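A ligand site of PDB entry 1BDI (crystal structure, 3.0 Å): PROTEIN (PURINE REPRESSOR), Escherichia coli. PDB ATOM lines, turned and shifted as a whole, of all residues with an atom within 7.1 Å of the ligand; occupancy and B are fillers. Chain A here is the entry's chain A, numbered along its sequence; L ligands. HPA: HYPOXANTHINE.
A nitrogen (N7) of the ligand lies within hydrogen-bond range of the side-chain hydroxyl (OG1) of Thr 191, 2.7 Å away.
N9 of the ligand is in hydrogen-bond range of OD2 of Asp 274.
NH2 of Arg 189 is in hydrogen-bond range of O6 of the ligand (3.0 Å).
O of Thr 191 sits close to NE of Arg 195 (3.4 Å).
The side-chain carboxylate (OD1) of Asp 274 lies within salt-bridge range of the guanidinium group (NH2) of Arg 195 (2.6 Å).
The backbone carbonyl oxygen of Asp 274 is in hydrogen-bond range of the backbone NH of Gln 291 (3.0 Å).
The backbone NH (N) of Asp 274 sits at hydrogen-bond distance from the side-chain carboxylate (OD1) of Asp 247 (3.3 Å).
The side-chain hydroxyl (OH) of Tyr 72 is in hydrogen-bond range of the side-chain amide oxygen (OE1) of Gln 291, at 2.7 Å.
NH2 of Arg 195 lies within hydrogen-bond range of OE1 of Gln 291.
The guanidinium group of Arg 195 is in hydrogen-bond range of the backbone carbonyl oxygen of Gly 245 (2.9 Å).
N of Arg 195 sits at hydrogen-bond distance from O of Asn 190 (3.4 Å).
Tyr 72 touches the ligand (CG to N9, 3.2 Å).
Phe 73 touches the ligand (CE2 to N1, 3.7 Å).
Arg 195 touches the ligand.
Phe 220 touches the ligand.
The nearest printed residue that does not touch the ligand is Ser 123 (4.1 Å).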
ATOM      1  N   THR A  66       6.115 -20.423  18.745  1.00  0.00           N
ATOM      2  CA  THR A  66       7.483 -20.877  18.853  1.00  0.00           C
ATOM      3  C   THR A  66       7.626 -22.266  18.329  1.00  0.00           C
ATOM      4  O   THR A  66       8.505 -22.555  17.519  1.00  0.00           O
ATOM      5  CB  THR A  66       7.975 -20.791  20.283  1.00  0.00           C
ATOM      6  OG1 THR A  66       8.162 -19.410  20.661  1.00  0.00           O
ATOM      7  CG2 THR A  66       9.263 -21.510  20.414  1.00  0.00           C
ATOM      8  N   SER A  67       6.739 -23.134  18.787  1.00  0.00           N
ATOM      9  CA  SER A  67       6.768 -24.525  18.359  1.00  0.00           C
ATOM     10  C   SER A  67       5.415 -25.147  18.780  1.00  0.00           C
ATOM     11  O   SER A  67       4.768 -24.684  19.704  1.00  0.00           O
ATOM     12  CB  SER A  67       8.015 -25.222  18.907  1.00  0.00           C
ATOM     13  OG  SER A  67       7.724 -26.266  19.810  1.00  0.00           O
ATOM     14  N   ALA A  70       5.446 -29.275  21.556  1.00  0.00           N
ATOM     15  CA  ALA A  70       5.479 -29.151  23.001  1.00  0.00           C
ATOM     16  C   ALA A  70       4.109 -29.161  23.647  1.00  0.00           C
ATOM     17  O   ALA A  70       3.221 -28.352  23.319  1.00  0.00           O
ATOM     18  CB  ALA A  70       6.201 -27.883  23.368  1.00  0.00           C
ATOM     19  N   ALA A  71       3.952 -30.105  24.543  1.00  0.00           N
ATOM     20  CA  ALA A  71       2.711 -30.275  25.292  1.00  0.00           C
ATOM     21  C   ALA A  71       2.028 -28.978  25.641  1.00  0.00           C
ATOM     22  O   ALA A  71       0.914 -28.732  25.192  1.00  0.00           O
ATOM     23  CB  ALA A  71       2.988 -31.096  26.552  1.00  0.00           C
ATOM     24  N   TYR A  72       2.742 -28.148  26.404  1.00  0.00           N
ATOM     25  CA  TYR A  72       2.237 -26.886  26.874  1.00  0.00           C
ATOM     26  C   TYR A  72       1.647 -26.149  25.703  1.00  0.00           C
ATOM     27  O   TYR A  72       0.420 -26.020  25.594  1.00  0.00           O
ATOM     28  CB  TYR A  72       3.391 -26.138  27.510  1.00  0.00           C
ATOM     29  CG  TYR A  72       3.143 -24.730  27.981  1.00  0.00           C
ATOM     30  CD1 TYR A  72       2.417 -24.468  29.119  1.00  0.00           C
ATOM     31  CD2 TYR A  72       3.715 -23.670  27.326  1.00  0.00           C
ATOM     32  CE1 TYR A  72       2.234 -23.146  29.574  1.00  0.00           C
ATOM     33  CE2 TYR A  72       3.551 -22.387  27.782  1.00  0.00           C
ATOM     34  CZ  TYR A  72       2.816 -22.118  28.890  1.00  0.00           C
ATOM     35  OH  TYR A  72       2.669 -20.802  29.257  1.00  0.00           O
ATOM     36  N   PHE A  73       2.518 -25.823  24.777  1.00  0.00           N
ATOM     37  CA  PHE A  73       2.152 -25.126  23.568  1.00  0.00           C
ATOM     38  C   PHE A  73       0.973 -25.654  22.855  1.00  0.00           C
ATOM     39  O   PHE A  73      -0.001 -24.970  22.535  1.00  0.00           O
ATOM     40  CB  PHE A  73       3.292 -25.275  22.641  1.00  0.00           C
ATOM     41  CG  PHE A  73       4.395 -24.381  23.025  1.00  0.00           C
ATOM     42  CD1 PHE A  73       4.087 -23.176  23.618  1.00  0.00           C
ATOM     43  CD2 PHE A  73       5.714 -24.738  22.838  1.00  0.00           C
ATOM     44  CE1 PHE A  73       5.080 -22.337  23.983  1.00  0.00           C
ATOM     45  CE2 PHE A  73       6.707 -23.899  23.202  1.00  0.00           C
ATOM     46  CZ  PHE A  73       6.392 -22.700  23.793  1.00  0.00           C
ATOM     47  N   ILE A  76      -2.312 -24.888  24.379  1.00  0.00           N
ATOM     48  CA  ILE A  76      -2.681 -23.503  24.194  1.00  0.00           C
ATOM     49  C   ILE A  76      -3.218 -23.342  22.758  1.00  0.00           C
ATOM     50  O   ILE A  76      -4.242 -22.729  22.519  1.00  0.00           O
ATOM     51  CB  ILE A  76      -1.508 -22.592  24.332  1.00  0.00           C
ATOM     52  CG1 ILE A  76      -1.100 -22.509  25.778  1.00  0.00           C
ATOM     53  CG2 ILE A  76      -1.921 -21.221  23.877  1.00  0.00           C
ATOM     54  CD1 ILE A  76       0.368 -22.850  26.026  1.00  0.00           C
ATOM     55  N   SER A 123       8.176 -16.712  23.248  1.00  0.00           N
ATOM     56  CA  SER A 123       9.082 -17.224  24.245  1.00  0.00           C
ATOM     57  C   SER A 123      10.161 -16.266  24.542  1.00  0.00           C
ATOM     58  O   SER A 123       9.981 -15.499  25.411  1.00  0.00           O
ATOM     59  CB  SER A 123       9.582 -18.608  23.892  1.00  0.00           C
ATOM     60  OG  SER A 123       8.462 -19.469  23.911  1.00  0.00           O
ATOM     61  N   GLU A 124      11.280 -16.247  23.848  1.00  0.00           N
ATOM     62  CA  GLU A 124      12.279 -15.220  24.206  1.00  0.00           C
ATOM     63  C   GLU A 124      11.841 -13.971  23.453  1.00  0.00           C
ATOM     64  O   GLU A 124      11.217 -14.103  22.402  1.00  0.00           O
ATOM     65  CB  GLU A 124      13.654 -15.592  23.657  1.00  0.00           C
ATOM     66  CG  GLU A 124      14.673 -16.058  24.651  1.00  0.00           C
ATOM     67  CD  GLU A 124      14.637 -17.534  24.777  1.00  0.00           C
ATOM     68  OE1 GLU A 124      13.493 -18.020  25.001  1.00  0.00           O
ATOM     69  OE2 GLU A 124      15.698 -18.190  24.623  1.00  0.00           O
ATOM     70  N   PRO A 186      14.391 -21.843  30.726  1.00  0.00           N
ATOM     71  CA  PRO A 186      15.268 -20.768  30.216  1.00  0.00           C
ATOM     72  C   PRO A 186      15.035 -19.426  30.924  1.00  0.00           C
ATOM     73  O   PRO A 186      13.896 -18.973  31.058  1.00  0.00           O
ATOM     74  CB  PRO A 186      14.877 -20.683  28.742  1.00  0.00           C
ATOM     75  CG  PRO A 186      14.343 -22.052  28.396  1.00  0.00           C
ATOM     76  CD  PRO A 186      13.982 -22.788  29.682  1.00  0.00           C
ATOM     77  N   ARG A 189      12.959 -16.454  29.523  1.00  0.00           N
ATOM     78  CA  ARG A 189      11.530 -16.692  29.411  1.00  0.00           C
ATOM     79  C   ARG A 189      10.812 -16.501  30.704  1.00  0.00           C
ATOM     80  O   ARG A 189      11.310 -16.819  31.776  1.00  0.00           O
ATOM     81  CB  ARG A 189      11.274 -18.118  28.952  1.00  0.00           C
ATOM     82  CG  ARG A 189      11.270 -18.277  27.467  1.00  0.00           C
ATOM     83  CD  ARG A 189      12.050 -19.477  27.109  1.00  0.00           C
ATOM     84  NE  ARG A 189      11.214 -20.494  26.492  1.00  0.00           N
ATOM     85  CZ  ARG A 189      11.628 -21.220  25.473  1.00  0.00           C
ATOM     86  NH1 ARG A 189      12.845 -20.991  25.003  1.00  0.00           N
ATOM     87  NH2 ARG A 189      10.859 -22.158  24.941  1.00  0.00           N
ATOM     88  N   ASN A 190       9.619 -15.967  30.599  1.00  0.00           N
ATOM     89  CA  ASN A 190       8.795 -15.693  31.758  1.00  0.00           C
ATOM     90  C   ASN A 190       8.576 -16.980  32.577  1.00  0.00           C
ATOM     91  O   ASN A 190       8.971 -17.068  33.773  1.00  0.00           O
ATOM     92  CB  ASN A 190       7.487 -15.106  31.263  1.00  0.00           C
ATOM     93  CG  ASN A 190       6.535 -14.896  32.361  1.00  0.00           C
ATOM     94  OD1 ASN A 190       6.832 -14.162  33.309  1.00  0.00           O
ATOM     95  ND2 ASN A 190       5.383 -15.572  32.290  1.00  0.00           N
ATOM     96  N   THR A 191       7.961 -17.967  31.917  1.00  0.00           N
ATOM     97  CA  THR A 191       7.698 -19.273  32.518  1.00  0.00           C
ATOM     98  C   THR A 191       9.005 -19.833  33.024  1.00  0.00           C
ATOM     99  O   THR A 191       8.993 -20.728  33.851  1.00  0.00           O
ATOM    100  CB  THR A 191       7.170 -20.268  31.505  1.00  0.00           C
ATOM    101  OG1 THR A 191       8.154 -20.435  30.485  1.00  0.00           O
ATOM    102  CG2 THR A 191       5.879 -19.768  30.901  1.00  0.00           C
ATOM    103  N   GLY A 192      10.130 -19.305  32.514  1.00  0.00           N
ATOM    104  CA  GLY A 192      11.440 -19.702  32.965  1.00  0.00           C
ATOM    105  C   GLY A 192      11.750 -18.854  34.223  1.00  0.00           C
ATOM    106  O   GLY A 192      11.405 -19.197  35.359  1.00  0.00           O
ATOM    107  N   ARG A 195       9.125 -17.966  37.076  1.00  0.00           N
ATOM    108  CA  ARG A 195       8.618 -19.019  37.916  1.00  0.00           C
ATOM    109  C   ARG A 195       9.661 -19.151  39.034  1.00  0.00           C
ATOM    110  O   ARG A 195       9.336 -19.078  40.229  1.00  0.00           O
ATOM    111  CB  ARG A 195       8.398 -20.286  37.074  1.00  0.00           C
ATOM    112  CG  ARG A 195       7.020 -20.344  36.371  1.00  0.00           C
ATOM    113  CD  ARG A 195       6.842 -21.557  35.435  1.00  0.00           C
ATOM    114  NE  ARG A 195       5.716 -21.467  34.504  1.00  0.00           N
ATOM    115  CZ  ARG A 195       5.299 -22.475  33.751  1.00  0.00           C
ATOM    116  NH1 ARG A 195       5.921 -23.643  33.848  1.00  0.00           N
ATOM    117  NH2 ARG A 195       4.277 -22.347  32.894  1.00  0.00           N
ATOM    118  N   ASP A 219      15.593 -26.925  29.561  1.00  0.00           N
ATOM    119  CA  ASP A 219      15.168 -26.211  28.362  1.00  0.00           C
ATOM    120  C   ASP A 219      13.689 -26.496  28.077  1.00  0.00           C
ATOM    121  O   ASP A 219      13.199 -26.221  26.967  1.00  0.00           O
ATOM    122  CB  ASP A 219      16.008 -26.693  27.198  1.00  0.00           C
ATOM    123  CG  ASP A 219      15.915 -28.173  26.986  1.00  0.00           C
ATOM    124  OD1 ASP A 219      15.132 -28.843  27.683  1.00  0.00           O
ATOM    125  OD2 ASP A 219      16.622 -28.699  26.121  1.00  0.00           O
ATOM    126  N   PHE A 220      13.007 -27.073  29.074  1.00  0.00           N
ATOM    127  CA  PHE A 220      11.572 -27.475  29.030  1.00  0.00           C
ATOM    128  C   PHE A 220      11.396 -28.821  28.336  1.00  0.00           C
ATOM    129  O   PHE A 220      10.270 -29.296  28.126  1.00  0.00           O
ATOM    130  CB  PHE A 220      10.650 -26.444  28.329  1.00  0.00           C
ATOM    131  CG  PHE A 220      10.267 -25.268  29.172  1.00  0.00           C
ATOM    132  CD1 PHE A 220       9.437 -25.400  30.247  1.00  0.00           C
ATOM    133  CD2 PHE A 220      10.749 -24.003  28.863  1.00  0.00           C
ATOM    134  CE1 PHE A 220       9.105 -24.318  31.019  1.00  0.00           C
ATOM    135  CE2 PHE A 220      10.400 -22.916  29.631  1.00  0.00           C
ATOM    136  CZ  PHE A 220       9.576 -23.089  30.711  1.00  0.00           C
ATOM    137  N   GLU A 221      12.518 -29.414  27.926  1.00  0.00           N
ATOM    138  CA  GLU A 221      12.439 -30.698  27.234  1.00  0.00           C
ATOM    139  C   GLU A 221      12.903 -31.830  28.132  1.00  0.00           C
ATOM    140  O   GLU A 221      13.933 -31.734  28.766  1.00  0.00           O
ATOM    141  CB  GLU A 221      13.188 -30.648  25.887  1.00  0.00           C
ATOM    142  CG  GLU A 221      12.729 -29.535  24.944  1.00  0.00           C
ATOM    143  CD  GLU A 221      11.978 -30.036  23.711  1.00  0.00           C
ATOM    144  OE1 GLU A 221      10.856 -30.566  23.862  1.00  0.00           O
ATOM    145  OE2 GLU A 221      12.505 -29.909  22.581  1.00  0.00           O
ATOM    146  N   GLY A 245      10.724 -26.702  36.889  1.00  0.00           N
ATOM    147  CA  GLY A 245      10.212 -25.622  36.061  1.00  0.00           C
ATOM    148  C   GLY A 245       8.982 -25.913  35.186  1.00  0.00           C
ATOM    149  O   GLY A 245       8.233 -24.996  34.897  1.00  0.00           O
ATOM    150  N   GLY A 246       8.792 -27.155  34.750  1.00  0.00           N
ATOM    151  CA  GLY A 246       7.650 -27.553  33.928  1.00  0.00           C
ATOM    152  C   GLY A 246       7.368 -29.089  33.891  1.00  0.00           C
ATOM    153  O   GLY A 246       8.296 -29.894  34.017  1.00  0.00           O
ATOM    154  N   ASP A 247       6.117 -29.483  33.688  1.00  0.00           N
ATOM    155  CA  ASP A 247       5.757 -30.903  33.629  1.00  0.00           C
ATOM    156  C   ASP A 247       6.520 -31.895  32.689  1.00  0.00           C
ATOM    157  O   ASP A 247       6.796 -33.027  33.070  1.00  0.00           O
ATOM    158  CB  ASP A 247       4.250 -31.080  33.474  1.00  0.00           C
ATOM    159  CG  ASP A 247       3.463 -30.403  34.593  1.00  0.00           C
ATOM    160  OD1 ASP A 247       4.068 -29.686  35.397  1.00  0.00           O
ATOM    161  OD2 ASP A 247       2.236 -30.612  34.688  1.00  0.00           O
ATOM    162  N   ILE A 248       6.872 -31.508  31.464  1.00  0.00           N
ATOM    163  CA  ILE A 248       7.575 -32.508  30.676  1.00  0.00           C
ATOM    164  C   ILE A 248       8.989 -32.714  31.182  1.00  0.00           C
ATOM    165  O   ILE A 248       9.501 -33.828  31.148  1.00  0.00           O
ATOM    166  CB  ILE A 248       7.626 -32.229  29.174  1.00  0.00           C
ATOM    167  CG1 ILE A 248       6.253 -31.850  28.595  1.00  0.00           C
ATOM    168  CG2 ILE A 248       8.288 -33.374  28.470  1.00  0.00           C
ATOM    169  CD1 ILE A 248       5.288 -32.935  28.598  1.00  0.00           C
ATOM    170  N   TYR A 273       5.293 -28.091  37.121  1.00  0.00           N
ATOM    171  CA  TYR A 273       4.544 -26.899  36.819  1.00  0.00           C
ATOM    172  C   TYR A 273       4.076 -26.884  35.384  1.00  0.00           C
ATOM    173  O   TYR A 273       4.894 -27.048  34.485  1.00  0.00           O
ATOM    174  CB  TYR A 273       5.438 -25.714  37.051  1.00  0.00           C
ATOM    175  CG  TYR A 273       4.720 -24.379  37.132  1.00  0.00           C
ATOM    176  CD1 TYR A 273       3.747 -24.032  36.224  1.00  0.00           C
ATOM    177  CD2 TYR A 273       5.068 -23.437  38.087  1.00  0.00           C
ATOM    178  CE1 TYR A 273       3.129 -22.801  36.274  1.00  0.00           C
ATOM    179  CE2 TYR A 273       4.457 -22.207  38.160  1.00  0.00           C
ATOM    180  CZ  TYR A 273       3.486 -21.878  37.251  1.00  0.00           C
ATOM    181  OH  TYR A 273       2.873 -20.631  37.326  1.00  0.00           O
ATOM    182  N   ASP A 274       2.746 -26.678  35.229  1.00  0.00           N
ATOM    183  CA  ASP A 274       1.968 -26.562  33.970  1.00  0.00           C
ATOM    184  C   ASP A 274       0.614 -27.260  34.066  1.00  0.00           C
ATOM    185  O   ASP A 274      -0.448 -26.767  33.644  1.00  0.00           O
ATOM    186  CB  ASP A 274       2.732 -27.093  32.752  1.00  0.00           C
ATOM    187  CG  ASP A 274       3.719 -26.053  32.169  1.00  0.00           C
ATOM    188  OD1 ASP A 274       3.878 -24.961  32.750  1.00  0.00           O
ATOM    189  OD2 ASP A 274       4.353 -26.290  31.114  1.00  0.00           O
ATOM    190  N   VAL A 276       0.039 -30.262  32.676  1.00  0.00           N
ATOM    191  CA  VAL A 276      -0.193 -30.697  31.315  1.00  0.00           C
ATOM    192  C   VAL A 276      -1.205 -31.840  31.205  1.00  0.00           C
ATOM    193  O   VAL A 276      -1.237 -32.733  32.043  1.00  0.00           O
ATOM    194  CB  VAL A 276       1.143 -30.949  30.624  1.00  0.00           C
ATOM    195  CG1 VAL A 276       1.062 -32.068  29.649  1.00  0.00           C
ATOM    196  CG2 VAL A 276       1.548 -29.691  29.928  1.00  0.00           C
ATOM    197  N   GLN A 291      -1.525 -24.384  35.051  1.00  0.00           N
ATOM    198  CA  GLN A 291      -1.650 -23.164  34.291  1.00  0.00           C
ATOM    199  C   GLN A 291      -2.858 -23.316  33.445  1.00  0.00           C
ATOM    200  O   GLN A 291      -3.011 -24.271  32.705  1.00  0.00           O
ATOM    201  CB  GLN A 291      -0.469 -22.921  33.382  1.00  0.00           C
ATOM    202  CG  GLN A 291      -0.691 -21.717  32.509  1.00  0.00           C
ATOM    203  CD  GLN A 291       0.578 -20.921  32.336  1.00  0.00           C
ATOM    204  OE1 GLN A 291       1.462 -21.338  31.594  1.00  0.00           O
ATOM    205  NE2 GLN A 291       0.684 -19.805  33.053  1.00  0.00           N
HETATM  206  N1  HPA L   1       8.105 -24.434  26.533  1.00  0.00           N
HETATM  207  C2  HPA L   1       7.455 -25.599  26.841  1.00  0.00           C
HETATM  208  N3  HPA L   1       6.666 -25.754  27.895  1.00  0.00           N
HETATM  209  C4  HPA L   1       6.563 -24.625  28.634  1.00  0.00           C
HETATM  210  C5  HPA L   1       7.171 -23.413  28.409  1.00  0.00           C
HETATM  211  C6  HPA L   1       8.015 -23.264  27.288  1.00  0.00           C
HETATM  212  O6  HPA L   1       8.654 -22.270  26.921  1.00  0.00           O
HETATM  213  N7  HPA L   1       6.831 -22.517  29.422  1.00  0.00           N
HETATM  214  C8  HPA L   1       6.032 -23.173  30.205  1.00  0.00           C
HETATM  215  N9  HPA L   1       5.797 -24.460  29.774  1.00  0.00           N
